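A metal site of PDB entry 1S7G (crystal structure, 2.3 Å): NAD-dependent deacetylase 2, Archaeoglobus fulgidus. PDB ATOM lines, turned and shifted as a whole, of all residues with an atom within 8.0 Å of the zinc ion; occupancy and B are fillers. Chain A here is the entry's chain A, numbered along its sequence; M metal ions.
Four residues have an atom within 4 Å of the zinc ion: Cys 126, Cys 129, Cys 150 and Cys 153.
The nearest printed residue that does not touch the zinc ion is Ser 155 (4.4 Å).
SG of Cys 129 is bound to the zinc ion.
SG of Cys 126 is bound to the zinc ion (2.4 Å).
SG of Cys 153 binds the zinc ion.
The zinc ion is bound by SG of Cys 150, at 2.4 Å.
The zinc ion has four donor atoms within binding distance.
The side-chain sulfur (SG) of Cys 150 sits close to the side-chain hydroxyl (OH) of Tyr 133 (3.0 Å).
The backbone NH of Lys 152 sits close to the side-chain sulfur of Cys 150, at 3.5 Å.
N of Ser 155 lies close to SG of Cys 153 (3.4 Å).
SG of Cys 129 lies close to N of Glu 131 (3.6 Å).
N of Cys 150 sits at hydrogen-bond distance from O of Ser 155, at 2.8 Å.
The backbone carbonyl oxygen (O) of Glu 131 sits at hydrogen-bond distance from the backbone NH (N) of Cys 126 (2.9 Å).
The backbone NH (N) of Asp 128 lies close to the side-chain sulfur (SG) of Cys 126.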
ATOM      1  N   ASP A 125       7.487 -16.160  35.267  1.00  0.00           N
ATOM      2  CA  ASP A 125       6.073 -16.308  34.930  1.00  0.00           C
ATOM      3  C   ASP A 125       5.643 -15.459  33.746  1.00  0.00           C
ATOM      4  O   ASP A 125       5.987 -14.273  33.654  1.00  0.00           O
ATOM      5  CB  ASP A 125       5.191 -15.909  36.131  1.00  0.00           C
ATOM      6  CG  ASP A 125       5.534 -16.683  37.394  1.00  0.00           C
ATOM      7  OD1 ASP A 125       5.257 -17.899  37.443  1.00  0.00           O
ATOM      8  OD2 ASP A 125       6.059 -16.059  38.337  1.00  0.00           O
ATOM      9  N   CYS A 126       4.887 -16.050  32.840  1.00  0.00           N
ATOM     10  CA  CYS A 126       4.369 -15.271  31.733  1.00  0.00           C
ATOM     11  C   CYS A 126       3.170 -14.532  32.329  1.00  0.00           C
ATOM     12  O   CYS A 126       2.267 -15.161  32.886  1.00  0.00           O
ATOM     13  CB  CYS A 126       3.871 -16.166  30.603  1.00  0.00           C
ATOM     14  SG  CYS A 126       2.946 -15.219  29.354  1.00  0.00           S
ATOM     15  N   LEU A 127       3.183 -13.215  32.219  1.00  0.00           N
ATOM     16  CA  LEU A 127       2.111 -12.377  32.755  1.00  0.00           C
ATOM     17  C   LEU A 127       0.807 -12.495  31.976  1.00  0.00           C
ATOM     18  O   LEU A 127      -0.251 -12.130  32.498  1.00  0.00           O
ATOM     19  CB  LEU A 127       2.550 -10.915  32.787  1.00  0.00           C
ATOM     20  CG  LEU A 127       3.144 -10.372  34.091  1.00  0.00           C
ATOM     21  CD1 LEU A 127       4.105 -11.342  34.703  1.00  0.00           C
ATOM     22  CD2 LEU A 127       3.814  -9.038  33.815  1.00  0.00           C
ATOM     23  N   ASP A 128       0.868 -13.004  30.749  1.00  0.00           N
ATOM     24  CA  ASP A 128      -0.341 -13.138  29.947  1.00  0.00           C
ATOM     25  C   ASP A 128      -1.065 -14.466  30.072  1.00  0.00           C
ATOM     26  O   ASP A 128      -2.273 -14.477  30.283  1.00  0.00           O
ATOM     27  CB  ASP A 128      -0.050 -12.841  28.475  1.00  0.00           C
ATOM     28  CG  ASP A 128       0.374 -11.405  28.237  1.00  0.00           C
ATOM     29  OD1 ASP A 128      -0.205 -10.501  28.863  1.00  0.00           O
ATOM     30  OD2 ASP A 128       1.293 -11.178  27.428  1.00  0.00           O
ATOM     31  N   CYS A 129      -0.356 -15.585  29.941  1.00  0.00           N
ATOM     32  CA  CYS A 129      -1.007 -16.890  30.050  1.00  0.00           C
ATOM     33  C   CYS A 129      -0.712 -17.674  31.342  1.00  0.00           C
ATOM     34  O   CYS A 129      -1.268 -18.754  31.566  1.00  0.00           O
ATOM     35  CB  CYS A 129      -0.657 -17.761  28.824  1.00  0.00           C
ATOM     36  SG  CYS A 129       0.895 -18.677  28.941  1.00  0.00           S
ATOM     37  N   HIS A 130       0.168 -17.144  32.176  1.00  0.00           N
ATOM     38  CA  HIS A 130       0.522 -17.750  33.459  1.00  0.00           C
ATOM     39  C   HIS A 130       1.390 -18.999  33.438  1.00  0.00           C
ATOM     40  O   HIS A 130       1.497 -19.692  34.451  1.00  0.00           O
ATOM     41  CB  HIS A 130      -0.739 -18.044  34.253  1.00  0.00           C
ATOM     42  CG  HIS A 130      -1.671 -16.880  34.300  1.00  0.00           C
ATOM     43  ND1 HIS A 130      -1.286 -15.662  34.829  1.00  0.00           N
ATOM     44  CD2 HIS A 130      -2.910 -16.709  33.802  1.00  0.00           C
ATOM     45  CE1 HIS A 130      -2.264 -14.784  34.652  1.00  0.00           C
ATOM     46  NE2 HIS A 130      -3.258 -15.391  34.031  1.00  0.00           N
ATOM     47  N   GLU A 131       1.989 -19.290  32.299  1.00  0.00           N
ATOM     48  CA  GLU A 131       2.877 -20.439  32.202  1.00  0.00           C
ATOM     49  C   GLU A 131       4.097 -20.102  33.064  1.00  0.00           C
ATOM     50  O   GLU A 131       4.498 -18.944  33.135  1.00  0.00           O
ATOM     51  CB  GLU A 131       3.319 -20.653  30.754  1.00  0.00           C
ATOM     52  CG  GLU A 131       4.124 -21.910  30.511  1.00  0.00           C
ATOM     53  CD  GLU A 131       3.311 -23.170  30.728  1.00  0.00           C
ATOM     54  OE1 GLU A 131       2.202 -23.260  30.144  1.00  0.00           O
ATOM     55  OE2 GLU A 131       3.765 -24.069  31.460  1.00  0.00           O
ATOM     56  N   THR A 132       4.668 -21.093  33.728  1.00  0.00           N
ATOM     57  CA  THR A 132       5.865 -20.831  34.528  1.00  0.00           C
ATOM     58  C   THR A 132       7.034 -21.606  33.955  1.00  0.00           C
ATOM     59  O   THR A 132       6.859 -22.718  33.454  1.00  0.00           O
ATOM     60  CB  THR A 132       5.666 -21.247  35.996  1.00  0.00           C
ATOM     61  OG1 THR A 132       5.433 -22.657  36.059  1.00  0.00           O
ATOM     62  CG2 THR A 132       4.497 -20.510  36.612  1.00  0.00           C
ATOM     63  N   TYR A 133       8.226 -21.019  34.009  1.00  0.00           N
ATOM     64  CA  TYR A 133       9.425 -21.652  33.493  1.00  0.00           C
ATOM     65  C   TYR A 133      10.564 -21.543  34.490  1.00  0.00           C
ATOM     66  O   TYR A 133      10.538 -20.695  35.392  1.00  0.00           O
ATOM     67  CB  TYR A 133       9.889 -20.978  32.207  1.00  0.00           C
ATOM     68  CG  TYR A 133       8.837 -20.888  31.118  1.00  0.00           C
ATOM     69  CD1 TYR A 133       8.004 -19.774  31.027  1.00  0.00           C
ATOM     70  CD2 TYR A 133       8.704 -21.911  30.184  1.00  0.00           C
ATOM     71  CE1 TYR A 133       7.051 -19.688  30.020  1.00  0.00           C
ATOM     72  CE2 TYR A 133       7.746 -21.833  29.179  1.00  0.00           C
ATOM     73  CZ  TYR A 133       6.928 -20.716  29.094  1.00  0.00           C
ATOM     74  OH  TYR A 133       5.987 -20.635  28.093  1.00  0.00           O
ATOM     75  N   ARG A 149      10.924 -15.161  25.781  1.00  0.00           N
ATOM     76  CA  ARG A 149       9.549 -15.074  25.281  1.00  0.00           C
ATOM     77  C   ARG A 149       8.816 -16.309  25.734  1.00  0.00           C
ATOM     78  O   ARG A 149       9.395 -17.387  25.816  1.00  0.00           O
ATOM     79  CB  ARG A 149       9.484 -15.040  23.754  1.00  0.00           C
ATOM     80  CG  ARG A 149       9.926 -13.757  23.073  1.00  0.00           C
ATOM     81  CD  ARG A 149       9.672 -13.890  21.566  1.00  0.00           C
ATOM     82  NE  ARG A 149       8.243 -13.941  21.241  1.00  0.00           N
ATOM     83  CZ  ARG A 149       7.746 -14.273  20.052  1.00  0.00           C
ATOM     84  NH1 ARG A 149       6.441 -14.287  19.840  1.00  0.00           N
ATOM     85  NH2 ARG A 149       8.558 -14.611  19.053  1.00  0.00           N
ATOM     86  N   CYS A 150       7.528 -16.172  25.997  1.00  0.00           N
ATOM     87  CA  CYS A 150       6.741 -17.322  26.411  1.00  0.00           C
ATOM     88  C   CYS A 150       6.627 -18.271  25.213  1.00  0.00           C
ATOM     89  O   CYS A 150       6.269 -17.857  24.109  1.00  0.00           O
ATOM     90  CB  CYS A 150       5.363 -16.882  26.871  1.00  0.00           C
ATOM     91  SG  CYS A 150       4.344 -18.254  27.409  1.00  0.00           S
ATOM     92  N   ARG A 151       6.925 -19.544  25.445  1.00  0.00           N
ATOM     93  CA  ARG A 151       6.853 -20.552  24.394  1.00  0.00           C
ATOM     94  C   ARG A 151       5.442 -21.061  24.116  1.00  0.00           C
ATOM     95  O   ARG A 151       5.188 -21.629  23.065  1.00  0.00           O
ATOM     96  CB  ARG A 151       7.751 -21.737  24.730  1.00  0.00           C
ATOM     97  CG  ARG A 151       9.228 -21.456  24.445  1.00  0.00           C
ATOM     98  CD  ARG A 151      10.142 -22.310  25.290  1.00  0.00           C
ATOM     99  NE  ARG A 151      11.560 -21.969  25.086  1.00  0.00           N
ATOM    100  CZ  ARG A 151      12.042 -20.721  25.050  1.00  0.00           C
ATOM    101  NH1 ARG A 151      11.232 -19.679  25.198  1.00  0.00           N
ATOM    102  NH2 ARG A 151      13.340 -20.513  24.883  1.00  0.00           N
ATOM    103  N   LYS A 152       4.521 -20.829  25.052  1.00  0.00           N
ATOM    104  CA  LYS A 152       3.151 -21.290  24.873  1.00  0.00           C
ATOM    105  C   LYS A 152       2.233 -20.260  24.223  1.00  0.00           C
ATOM    106  O   LYS A 152       1.374 -20.635  23.427  1.00  0.00           O
ATOM    107  CB  LYS A 152       2.572 -21.742  26.221  1.00  0.00           C
ATOM    108  N   CYS A 153       2.406 -18.978  24.536  1.00  0.00           N
ATOM    109  CA  CYS A 153       1.551 -17.945  23.959  1.00  0.00           C
ATOM    110  C   CYS A 153       2.315 -16.898  23.144  1.00  0.00           C
ATOM    111  O   CYS A 153       1.721 -16.084  22.443  1.00  0.00           O
ATOM    112  CB  CYS A 153       0.727 -17.250  25.041  1.00  0.00           C
ATOM    113  SG  CYS A 153       1.593 -15.946  25.938  1.00  0.00           S
ATOM    114  N   GLY A 154       3.648 -16.905  23.251  1.00  0.00           N
ATOM    115  CA  GLY A 154       4.445 -15.961  22.493  1.00  0.00           C
ATOM    116  C   GLY A 154       4.610 -14.572  23.102  1.00  0.00           C
ATOM    117  O   GLY A 154       5.148 -13.674  22.468  1.00  0.00           O
ATOM    118  N   SER A 155       4.157 -14.406  24.344  1.00  0.00           N
ATOM    119  CA  SER A 155       4.261 -13.125  25.042  1.00  0.00           C
ATOM    120  C   SER A 155       5.702 -12.749  25.433  1.00  0.00           C
ATOM    121  O   SER A 155       6.541 -13.620  25.679  1.00  0.00           O
ATOM    122  CB  SER A 155       3.393 -13.178  26.302  1.00  0.00           C
ATOM    123  OG  SER A 155       3.644 -12.058  27.147  1.00  0.00           O
ATOM    124  N   TYR A 156       5.969 -11.450  25.490  1.00  0.00           N
ATOM    125  CA  TYR A 156       7.292 -10.975  25.886  1.00  0.00           C
ATOM    126  C   TYR A 156       7.237 -10.520  27.336  1.00  0.00           C
ATOM    127  O   TYR A 156       8.146  -9.839  27.803  1.00  0.00           O
ATOM    128  CB  TYR A 156       7.757  -9.792  25.020  1.00  0.00           C
ATOM    129  CG  TYR A 156       8.080 -10.145  23.588  1.00  0.00           C
ATOM    130  CD1 TYR A 156       7.071 -10.273  22.643  1.00  0.00           C
ATOM    131  CD2 TYR A 156       9.400 -10.338  23.190  1.00  0.00           C
ATOM    132  CE1 TYR A 156       7.364 -10.576  21.325  1.00  0.00           C
ATOM    133  CE2 TYR A 156       9.708 -10.653  21.867  1.00  0.00           C
ATOM    134  CZ  TYR A 156       8.686 -10.769  20.936  1.00  0.00           C
ATOM    135  OH  TYR A 156       8.980 -11.059  19.628  1.00  0.00           O
ATOM    136  N   TYR A 157       6.176 -10.880  28.031  1.00  0.00           N
ATOM    137  CA  TYR A 157       6.006 -10.511  29.430  1.00  0.00           C
ATOM    138  C   TYR A 157       6.311 -11.674  30.365  1.00  0.00           C
ATOM    139  O   TYR A 157       5.437 -12.157  31.085  1.00  0.00           O
ATOM    140  CB  TYR A 157       4.585  -9.988  29.689  1.00  0.00           C
ATOM    141  CG  TYR A 157       4.253  -8.725  28.929  1.00  0.00           C
ATOM    142  CD1 TYR A 157       3.921  -8.755  27.583  1.00  0.00           C
ATOM    143  CD2 TYR A 157       4.326  -7.478  29.565  1.00  0.00           C
ATOM    144  CE1 TYR A 157       3.650  -7.575  26.880  1.00  0.00           C
ATOM    145  CE2 TYR A 157       4.058  -6.297  28.871  1.00  0.00           C
ATOM    146  CZ  TYR A 157       3.731  -6.355  27.525  1.00  0.00           C
ATOM    147  OH  TYR A 157       3.507  -5.188  26.838  1.00  0.00           O
ATOM    148  N   VAL A 158       7.560 -12.135  30.343  1.00  0.00           N
ATOM    149  CA  VAL A 158       7.970 -13.225  31.205  1.00  0.00           C
ATOM    150  C   VAL A 158       8.748 -12.563  32.344  1.00  0.00           C
ATOM    151  O   VAL A 158       9.903 -12.181  32.177  1.00  0.00           O
ATOM    152  CB  VAL A 158       8.860 -14.238  30.444  1.00  0.00           C
ATOM    153  CG1 VAL A 158       9.204 -15.408  31.355  1.00  0.00           C
ATOM    154  CG2 VAL A 158       8.120 -14.732  29.210  1.00  0.00           C
HETATM  155 ZN    ZN M   1       2.286 -17.049  27.964  1.00  0.00          ZN
